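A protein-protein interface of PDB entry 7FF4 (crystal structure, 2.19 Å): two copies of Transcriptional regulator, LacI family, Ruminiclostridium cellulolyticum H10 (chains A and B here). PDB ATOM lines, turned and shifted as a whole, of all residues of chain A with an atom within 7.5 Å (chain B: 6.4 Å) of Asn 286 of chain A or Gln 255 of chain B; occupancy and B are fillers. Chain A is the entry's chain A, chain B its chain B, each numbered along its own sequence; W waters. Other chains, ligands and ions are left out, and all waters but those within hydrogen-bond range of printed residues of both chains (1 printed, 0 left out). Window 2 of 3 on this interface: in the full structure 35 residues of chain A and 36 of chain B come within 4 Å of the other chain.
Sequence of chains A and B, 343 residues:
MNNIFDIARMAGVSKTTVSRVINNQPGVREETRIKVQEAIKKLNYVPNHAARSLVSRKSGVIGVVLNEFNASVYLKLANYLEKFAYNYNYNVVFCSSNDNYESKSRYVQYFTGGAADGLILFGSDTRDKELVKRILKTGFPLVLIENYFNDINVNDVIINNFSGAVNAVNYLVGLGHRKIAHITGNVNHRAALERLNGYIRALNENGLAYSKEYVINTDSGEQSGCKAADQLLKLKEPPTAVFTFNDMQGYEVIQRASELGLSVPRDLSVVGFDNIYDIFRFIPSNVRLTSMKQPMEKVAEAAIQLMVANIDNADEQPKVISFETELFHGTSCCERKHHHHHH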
ATOM      1  N   ILE A 254      23.387   2.828 -14.944  1.00  0.00           N
ATOM      2  CA  ILE A 254      22.536   3.946 -15.426  1.00  0.00           C
ATOM      3  C   ILE A 254      23.062   4.426 -16.780  1.00  0.00           C
ATOM      4  O   ILE A 254      22.261   4.619 -17.669  1.00  0.00           O
ATOM      5  CB  ILE A 254      22.506   5.075 -14.384  1.00  0.00           C
ATOM      6  CG1 ILE A 254      21.612   4.719 -13.200  1.00  0.00           C
ATOM      7  CG2 ILE A 254      22.089   6.383 -15.014  1.00  0.00           C
ATOM      8  CD1 ILE A 254      21.880   5.518 -11.977  1.00  0.00           C
ATOM      9  N   VAL A 264      16.434   5.832 -16.965  1.00  0.00           N
ATOM     10  CA  VAL A 264      16.406   5.433 -15.532  1.00  0.00           C
ATOM     11  C   VAL A 264      15.776   6.590 -14.773  1.00  0.00           C
ATOM     12  O   VAL A 264      16.159   7.687 -15.052  1.00  0.00           O
ATOM     13  CB  VAL A 264      17.827   5.185 -15.007  1.00  0.00           C
ATOM     14  CG1 VAL A 264      17.846   5.009 -13.507  1.00  0.00           C
ATOM     15  CG2 VAL A 264      18.480   4.008 -15.688  1.00  0.00           C
ATOM     16  N   TYR A 277      28.096   9.516  -3.396  1.00  0.00           N
ATOM     17  CA  TYR A 277      27.799  10.912  -3.763  1.00  0.00           C
ATOM     18  C   TYR A 277      28.202  11.823  -2.612  1.00  0.00           C
ATOM     19  O   TYR A 277      28.559  12.952  -2.848  1.00  0.00           O
ATOM     20  CB  TYR A 277      26.304  11.010  -4.018  1.00  0.00           C
ATOM     21  CG  TYR A 277      25.883  12.087  -4.965  1.00  0.00           C
ATOM     22  CD1 TYR A 277      25.683  11.812  -6.300  1.00  0.00           C
ATOM     23  CD2 TYR A 277      25.634  13.364  -4.509  1.00  0.00           C
ATOM     24  CE1 TYR A 277      25.250  12.789  -7.172  1.00  0.00           C
ATOM     25  CE2 TYR A 277      25.219  14.360  -5.369  1.00  0.00           C
ATOM     26  CZ  TYR A 277      25.021  14.068  -6.703  1.00  0.00           C
ATOM     27  OH  TYR A 277      24.609  15.049  -7.552  1.00  0.00           O
ATOM     28  N   ILE A 283      27.528  18.280  -8.070  1.00  0.00           N
ATOM     29  CA  ILE A 283      26.342  17.550  -8.610  1.00  0.00           C
ATOM     30  C   ILE A 283      26.582  17.146 -10.064  1.00  0.00           C
ATOM     31  O   ILE A 283      26.152  17.869 -10.948  1.00  0.00           O
ATOM     32  CB  ILE A 283      25.097  18.444  -8.499  1.00  0.00           C
ATOM     33  CG1 ILE A 283      24.767  18.761  -7.041  1.00  0.00           C
ATOM     34  CG2 ILE A 283      23.920  17.825  -9.227  1.00  0.00           C
ATOM     35  CD1 ILE A 283      24.340  20.183  -6.811  1.00  0.00           C
ATOM     36  N   PRO A 284      27.222  15.918 -10.460  1.00  0.00           N
ATOM     37  CA  PRO A 284      27.645  15.159 -11.906  1.00  0.00           C
ATOM     38  C   PRO A 284      26.350  14.945 -12.693  1.00  0.00           C
ATOM     39  O   PRO A 284      26.325  15.245 -13.838  1.00  0.00           O
ATOM     40  CB  PRO A 284      28.323  13.866 -11.479  1.00  0.00           C
ATOM     41  CG  PRO A 284      27.749  13.607 -10.125  1.00  0.00           C
ATOM     42  CD  PRO A 284      27.681  14.960  -9.459  1.00  0.00           C
ATOM     43  N   SER A 285      25.277  14.537 -12.013  1.00  0.00           N
ATOM     44  CA  SER A 285      24.035  14.163 -12.732  1.00  0.00           C
ATOM     45  C   SER A 285      22.771  14.425 -11.914  1.00  0.00           C
ATOM     46  O   SER A 285      22.873  14.620 -10.716  1.00  0.00           O
ATOM     47  CB  SER A 285      24.110  12.718 -13.097  1.00  0.00           C
ATOM     48  OG  SER A 285      22.828  12.226 -13.388  1.00  0.00           O
ATOM     49  N   ASN A 286      21.620  14.388 -12.577  1.00  0.00           N
ATOM     50  CA  ASN A 286      20.303  14.609 -11.929  1.00  0.00           C
ATOM     51  C   ASN A 286      19.815  13.282 -11.351  1.00  0.00           C
ATOM     52  O   ASN A 286      18.869  13.305 -10.571  1.00  0.00           O
ATOM     53  CB  ASN A 286      19.255  15.078 -12.933  1.00  0.00           C
ATOM     54  CG  ASN A 286      19.060  14.072 -14.043  1.00  0.00           C
ATOM     55  OD1 ASN A 286      20.020  13.479 -14.521  1.00  0.00           O
ATOM     56  ND2 ASN A 286      17.823  13.878 -14.454  1.00  0.00           N
ATOM     57  N   VAL A 287      20.418  12.179 -11.787  1.00  0.00           N
ATOM     58  CA  VAL A 287      20.030  10.853 -11.245  1.00  0.00           C
ATOM     59  C   VAL A 287      21.022  10.473 -10.161  1.00  0.00           C
ATOM     60  O   VAL A 287      22.111  10.062 -10.488  1.00  0.00           O
ATOM     61  CB  VAL A 287      19.946   9.761 -12.316  1.00  0.00           C
ATOM     62  CG1 VAL A 287      19.549   8.447 -11.686  1.00  0.00           C
ATOM     63  CG2 VAL A 287      18.958  10.136 -13.396  1.00  0.00           C
ATOM     64  N   ARG A 288      20.630  10.654  -8.910  1.00  0.00           N
ATOM     65  CA  ARG A 288      21.484  10.242  -7.781  1.00  0.00           C
ATOM     66  C   ARG A 288      20.973   8.884  -7.317  1.00  0.00           C
ATOM     67  O   ARG A 288      19.785   8.709  -7.225  1.00  0.00           O
ATOM     68  CB  ARG A 288      21.467  11.252  -6.639  1.00  0.00           C
ATOM     69  CG  ARG A 288      22.328  10.834  -5.461  1.00  0.00           C
ATOM     70  CD  ARG A 288      22.312  11.824  -4.336  1.00  0.00           C
ATOM     71  NE  ARG A 288      22.965  11.330  -3.155  1.00  0.00           N
ATOM     72  CZ  ARG A 288      23.268  12.061  -2.110  1.00  0.00           C
ATOM     73  NH1 ARG A 288      22.975  13.341  -2.098  1.00  0.00           N
ATOM     74  NH2 ARG A 288      23.852  11.516  -1.070  1.00  0.00           N
ATOM     75  N   LEU A 289      21.891   7.986  -7.029  1.00  0.00           N
ATOM     76  CA  LEU A 289      21.553   6.612  -6.618  1.00  0.00           C
ATOM     77  C   LEU A 289      20.889   6.544  -5.251  1.00  0.00           C
ATOM     78  O   LEU A 289      21.398   7.101  -4.317  1.00  0.00           O
ATOM     79  CB  LEU A 289      22.847   5.809  -6.541  1.00  0.00           C
ATOM     80  CG  LEU A 289      23.325   5.185  -7.839  1.00  0.00           C
ATOM     81  CD1 LEU A 289      24.563   4.359  -7.598  1.00  0.00           C
ATOM     82  CD2 LEU A 289      22.233   4.358  -8.472  1.00  0.00           C
ATOM     83  N   GLY A 330      17.422   8.385  -3.200  1.00  0.00           N
ATOM     84  CA  GLY A 330      17.859   9.265  -4.290  1.00  0.00           C
ATOM     85  C   GLY A 330      16.800   9.397  -5.362  1.00  0.00           C
ATOM     86  O   GLY A 330      15.647   9.415  -5.037  1.00  0.00           O
ATOM     87  N   THR A 331      17.208   9.479  -6.614  1.00  0.00           N
ATOM     88  CA  THR A 331      16.227   9.658  -7.702  1.00  0.00           C
ATOM     89  C   THR A 331      16.374   8.538  -8.730  1.00  0.00           C
ATOM     90  O   THR A 331      15.908   8.714  -9.828  1.00  0.00           O
ATOM     91  CB  THR A 331      16.356  11.067  -8.287  1.00  0.00           C
ATOM     92  OG1 THR A 331      17.680  11.204  -8.784  1.00  0.00           O
ATOM     93  CG2 THR A 331      16.109  12.153  -7.268  1.00  0.00           C
ATOM     94  N   SER A 332      16.956   7.411  -8.334  1.00  0.00           N
ATOM     95  CA  SER A 332      17.195   6.284  -9.267  1.00  0.00           C
ATOM     96  C   SER A 332      16.126   5.196  -9.169  1.00  0.00           C
ATOM     97  O   SER A 332      16.305   4.180  -9.792  1.00  0.00           O
ATOM     98  CB  SER A 332      18.542   5.712  -9.045  1.00  0.00           C
ATOM     99  OG  SER A 332      18.717   5.359  -7.698  1.00  0.00           O
ATOM    100  N   CYS B 226      26.045  24.791 -12.680  1.00  0.00           N
ATOM    101  CA  CYS B 226      24.624  24.772 -13.106  1.00  0.00           C
ATOM    102  C   CYS B 226      24.125  26.179 -13.411  1.00  0.00           C
ATOM    103  O   CYS B 226      23.610  26.381 -14.482  1.00  0.00           O
ATOM    104  CB  CYS B 226      23.744  24.159 -12.028  1.00  0.00           C
ATOM    105  SG  CYS B 226      24.059  22.397 -11.788  1.00  0.00           S
ATOM    106  N   GLY B 250      32.535  21.600 -14.959  1.00  0.00           N
ATOM    107  CA  GLY B 250      32.296  21.021 -16.287  1.00  0.00           C
ATOM    108  C   GLY B 250      31.147  20.039 -16.279  1.00  0.00           C
ATOM    109  O   GLY B 250      30.285  20.151 -17.120  1.00  0.00           O
ATOM    110  N   TYR B 251      31.156  19.103 -15.339  1.00  0.00           N
ATOM    111  CA  TYR B 251      30.087  18.082 -15.239  1.00  0.00           C
ATOM    112  C   TYR B 251      28.742  18.766 -14.972  1.00  0.00           C
ATOM    113  O   TYR B 251      27.768  18.415 -15.595  1.00  0.00           O
ATOM    114  CB  TYR B 251      30.504  16.978 -14.265  1.00  0.00           C
ATOM    115  CG  TYR B 251      31.564  16.067 -14.820  1.00  0.00           C
ATOM    116  CD1 TYR B 251      31.319  15.328 -15.952  1.00  0.00           C
ATOM    117  CD2 TYR B 251      32.815  15.975 -14.250  1.00  0.00           C
ATOM    118  CE1 TYR B 251      32.272  14.505 -16.501  1.00  0.00           C
ATOM    119  CE2 TYR B 251      33.780  15.149 -14.783  1.00  0.00           C
ATOM    120  CZ  TYR B 251      33.508  14.412 -15.912  1.00  0.00           C
ATOM    121  OH  TYR B 251      34.441  13.602 -16.463  1.00  0.00           O
ATOM    122  N   GLU B 252      28.741  19.769 -14.107  1.00  0.00           N
ATOM    123  CA  GLU B 252      27.521  20.533 -13.778  1.00  0.00           C
ATOM    124  C   GLU B 252      27.030  21.247 -15.034  1.00  0.00           C
ATOM    125  O   GLU B 252      25.834  21.362 -15.188  1.00  0.00           O
ATOM    126  CB  GLU B 252      27.777  21.509 -12.634  1.00  0.00           C
ATOM    127  CG  GLU B 252      27.876  20.826 -11.293  1.00  0.00           C
ATOM    128  CD  GLU B 252      28.167  21.717 -10.106  1.00  0.00           C
ATOM    129  OE1 GLU B 252      28.619  22.833 -10.303  1.00  0.00           O
ATOM    130  OE2 GLU B 252      27.947  21.278  -8.993  1.00  0.00           O
ATOM    131  N   VAL B 253      27.948  21.708 -15.882  1.00  0.00           N
ATOM    132  CA  VAL B 253      27.558  22.391 -17.144  1.00  0.00           C
ATOM    133  C   VAL B 253      26.850  21.381 -18.036  1.00  0.00           C
ATOM    134  O   VAL B 253      25.830  21.715 -18.594  1.00  0.00           O
ATOM    135  CB  VAL B 253      28.760  22.996 -17.885  1.00  0.00           C
ATOM    136  CG1 VAL B 253      28.449  23.210 -19.349  1.00  0.00           C
ATOM    137  CG2 VAL B 253      29.240  24.275 -17.240  1.00  0.00           C
ATOM    138  N   ILE B 254      27.405  20.185 -18.144  1.00  0.00           N
ATOM    139  CA  ILE B 254      26.800  19.133 -19.000  1.00  0.00           C
ATOM    140  C   ILE B 254      25.400  18.802 -18.471  1.00  0.00           C
ATOM    141  O   ILE B 254      24.499  18.643 -19.276  1.00  0.00           O
ATOM    142  CB  ILE B 254      27.723  17.906 -19.058  1.00  0.00           C
ATOM    143  CG1 ILE B 254      28.959  18.188 -19.911  1.00  0.00           C
ATOM    144  CG2 ILE B 254      26.972  16.700 -19.563  1.00  0.00           C
ATOM    145  CD1 ILE B 254      30.208  17.516 -19.442  1.00  0.00           C
ATOM    146  N   GLN B 255      25.246  18.737 -17.155  1.00  0.00           N
ATOM    147  CA  GLN B 255      23.950  18.403 -16.527  1.00  0.00           C
ATOM    148  C   GLN B 255      22.918  19.480 -16.858  1.00  0.00           C
ATOM    149  O   GLN B 255      21.873  19.123 -17.349  1.00  0.00           O
ATOM    150  CB  GLN B 255      24.144  18.208 -15.026  1.00  0.00           C
ATOM    151  CG  GLN B 255      22.874  17.911 -14.254  1.00  0.00           C
ATOM    152  CD  GLN B 255      22.048  16.818 -14.880  1.00  0.00           C
ATOM    153  OE1 GLN B 255      22.561  15.894 -15.493  1.00  0.00           O
ATOM    154  NE2 GLN B 255      20.745  16.920 -14.719  1.00  0.00           N
ATOM    155  N   ARG B 256      23.232  20.746 -16.613  1.00  0.00           N
ATOM    156  CA  ARG B 256      22.261  21.834 -16.878  1.00  0.00           C
ATOM    157  C   ARG B 256      21.922  21.911 -18.364  1.00  0.00           C
ATOM    158  O   ARG B 256      20.782  22.207 -18.681  1.00  0.00           O
ATOM    159  CB  ARG B 256      22.794  23.179 -16.397  1.00  0.00           C
ATOM    160  CG  ARG B 256      21.794  24.307 -16.554  1.00  0.00           C
ATOM    161  CD  ARG B 256      20.399  23.869 -16.188  1.00  0.00           C
ATOM    162  NE  ARG B 256      19.495  24.987 -16.048  1.00  0.00           N
ATOM    163  CZ  ARG B 256      18.182  24.881 -15.991  1.00  0.00           C
ATOM    164  NH1 ARG B 256      17.611  23.697 -16.064  1.00  0.00           N
ATOM    165  NH2 ARG B 256      17.437  25.954 -15.868  1.00  0.00           N
ATOM    166  N   ALA B 257      22.899  21.669 -19.229  1.00  0.00           N
ATOM    167  CA  ALA B 257      22.679  21.727 -20.685  1.00  0.00           C
ATOM    168  C   ALA B 257      21.653  20.671 -21.080  1.00  0.00           C
ATOM    169  O   ALA B 257      20.740  20.989 -21.808  1.00  0.00           O
ATOM    170  CB  ALA B 257      23.975  21.521 -21.399  1.00  0.00           C
ATOM    171  N   SER B 258      21.833  19.448 -20.601  1.00  0.00           N
ATOM    172  CA  SER B 258      20.916  18.343 -20.955  1.00  0.00           C
ATOM    173  C   SER B 258      19.523  18.655 -20.420  1.00  0.00           C
ATOM    174  O   SER B 258      18.566  18.334 -21.084  1.00  0.00           O
ATOM    175  CB  SER B 258      21.436  17.038 -20.475  1.00  0.00           C
ATOM    176  OG  SER B 258      20.835  16.689 -19.248  1.00  0.00           O
ATOM    177  N   GLU B 259      19.445  19.325 -19.278  1.00  0.00           N
ATOM    178  CA  GLU B 259      18.147  19.741 -18.704  1.00  0.00           C
ATOM    179  C   GLU B 259      17.497  20.743 -19.661  1.00  0.00           C
ATOM    180  O   GLU B 259      16.277  20.785 -19.736  1.00  0.00           O
ATOM    181  CB  GLU B 259      18.348  20.387 -17.338  1.00  0.00           C
ATOM    182  CG  GLU B 259      18.677  19.391 -16.258  1.00  0.00           C
ATOM    183  CD  GLU B 259      18.914  19.996 -14.894  1.00  0.00           C
ATOM    184  OE1 GLU B 259      18.728  21.192 -14.752  1.00  0.00           O
ATOM    185  OE2 GLU B 259      19.287  19.262 -13.997  1.00  0.00           O
ATOM    186  N   LEU B 260      18.306  21.498 -20.397  1.00  0.00           N
ATOM    187  CA  LEU B 260      17.765  22.493 -21.348  1.00  0.00           C
ATOM    188  C   LEU B 260      17.626  21.858 -22.726  1.00  0.00           C
ATOM    189  O   LEU B 260      17.356  22.574 -23.658  1.00  0.00           O
ATOM    190  CB  LEU B 260      18.679  23.717 -21.390  1.00  0.00           C
ATOM    191  CG  LEU B 260      18.661  24.579 -20.139  1.00  0.00           C
ATOM    192  CD1 LEU B 260      19.745  25.625 -20.197  1.00  0.00           C
ATOM    193  CD2 LEU B 260      17.310  25.228 -19.953  1.00  0.00           C
ATOM    194  N   PRO B 284      29.419  10.120 -12.984  1.00  0.00           N
ATOM    195  CA  PRO B 284      28.046   9.828 -13.339  1.00  0.00           C
ATOM    196  C   PRO B 284      27.678  10.936 -14.326  1.00  0.00           C
ATOM    197  O   PRO B 284      27.211  11.947 -13.943  1.00  0.00           O
ATOM    198  CB  PRO B 284      27.253  10.032 -12.048  1.00  0.00           C
ATOM    199  CG  PRO B 284      28.285   9.975 -10.952  1.00  0.00           C
ATOM    200  CD  PRO B 284      29.544  10.521 -11.575  1.00  0.00           C
ATOM    201  N   SER B 285      27.938  10.660 -15.593  1.00  0.00           N
ATOM    202  CA  SER B 285      27.687  11.590 -16.713  1.00  0.00           C
ATOM    203  C   SER B 285      27.796  10.796 -18.007  1.00  0.00           C
ATOM    204  O   SER B 285      28.474   9.782 -18.024  1.00  0.00           O
ATOM    205  CB  SER B 285      28.676  12.717 -16.699  1.00  0.00           C
ATOM    206  OG  SER B 285      28.400  13.635 -17.727  1.00  0.00           O
HETATM  207  O   HOH W   1      27.469  15.819 -16.175  1.00  0.00           O
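Hydrophobic or aromatic side chains of chain B within 4 Å of the printed part of chain A: Pro 284.
Among the printed residues, 7 pairs touch across the chains.
Among the printed residues, no Asp or Glu carboxylate lies within 4 Å of a Lys or Arg side-chain nitrogen of the other chain.
Water W1 lies within hydrogen-bond range of O of Pro 284 of chain A, O of Tyr 251 of chain B and OG of Ser 285 of chain B.
The side-chain hydroxyl (OG1) of Thr 331 of chain A sits at hydrogen-bond distance from the backbone carbonyl oxygen (O) of Asn 286 of chain A (3.0 Å).
O of Gln 255 of chain B sits at hydrogen-bond distance from OG of Ser 258 of chain B (3.3 Å).
The side-chain hydroxyl of Ser 285 of chain A sits at hydrogen-bond distance from the side-chain amide oxygen of Asn 286 of chain A, 3.3 Å away.
The side-chain hydroxyl (OG) of Ser 285 of chain A sits at hydrogen-bond distance from the backbone NH (N) of Val 287 of chain A, at 2.9 Å.
The side-chain amide nitrogen of Gln 255 of chain B sits at hydrogen-bond distance from the side-chain carboxylate of Glu 259 of chain B, 2.9 Å away.
Of the printed residues of chain B, Ser 285 of chain A touches Gln 255 (3.6 Å) and Pro 284 (3.3 Å).
Of the printed residues of chain B, Asn 286 of chain A touches Gln 255 (3.0 Å).
Leu 289 of chain A touches none of the printed residues of chain B.
Of the printed residues of chain A, Glu 252 of chain B touches Ile 283 (3.2 Å).
Gln 255 of chain B touches three residues of chain A.
The nearest residue of chain B that does not touch Asn 286 of chain A is Glu 259 of chain B (4.3 Å).
The nearest residue of chain A that does not touch Gln 255 of chain B is Ile 283 of chain A (4.6 Å).
The nearest printed residue of chain B that does not touch Ser 285 of chain A is Ser 285 of chain B (5.0 Å).
Pro 284 of chain A touches its own counterpart, Pro 284 of chain B.
Ser 285 of chain A touches Pro 284 of chain B, but with the chains exchanged Pro 284 of chain A does not touch Ser 285 of chain B (4.5 Å).
Positions printed for both chains: 254, 284 and 285.
Of the 7 pairs that touch across the chains among the printed residues, 1 has its exchanged pair printed and touching as well.
The backbone carbonyl oxygen of Pro 284 of chain B sits close to the backbone carbonyl oxygen of Pro 284 of chain A (3.4 Å).
The side-chain amide oxygen of Gln 255 of chain B lies close to the backbone NH of Asn 286 of chain A (3.4 Å).
The backbone NH (N) of Ile 283 of chain A lies within hydrogen-bond range of the side-chain carboxylate (OE2) of Glu 252 of chain B, 3.2 Å away.
Among the printed residues, merely in contact across the chains: Ser 285 of chain A with Pro 284 of chain B (3.3 Å), Ser 285 of chain A with Gln 255 of chain B (3.6 Å), Pro 284 of chain A with Gln 255 of chain B (3.9 Å) and Pro 284 of chain A with Tyr 251 of chain B (3.9 Å).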
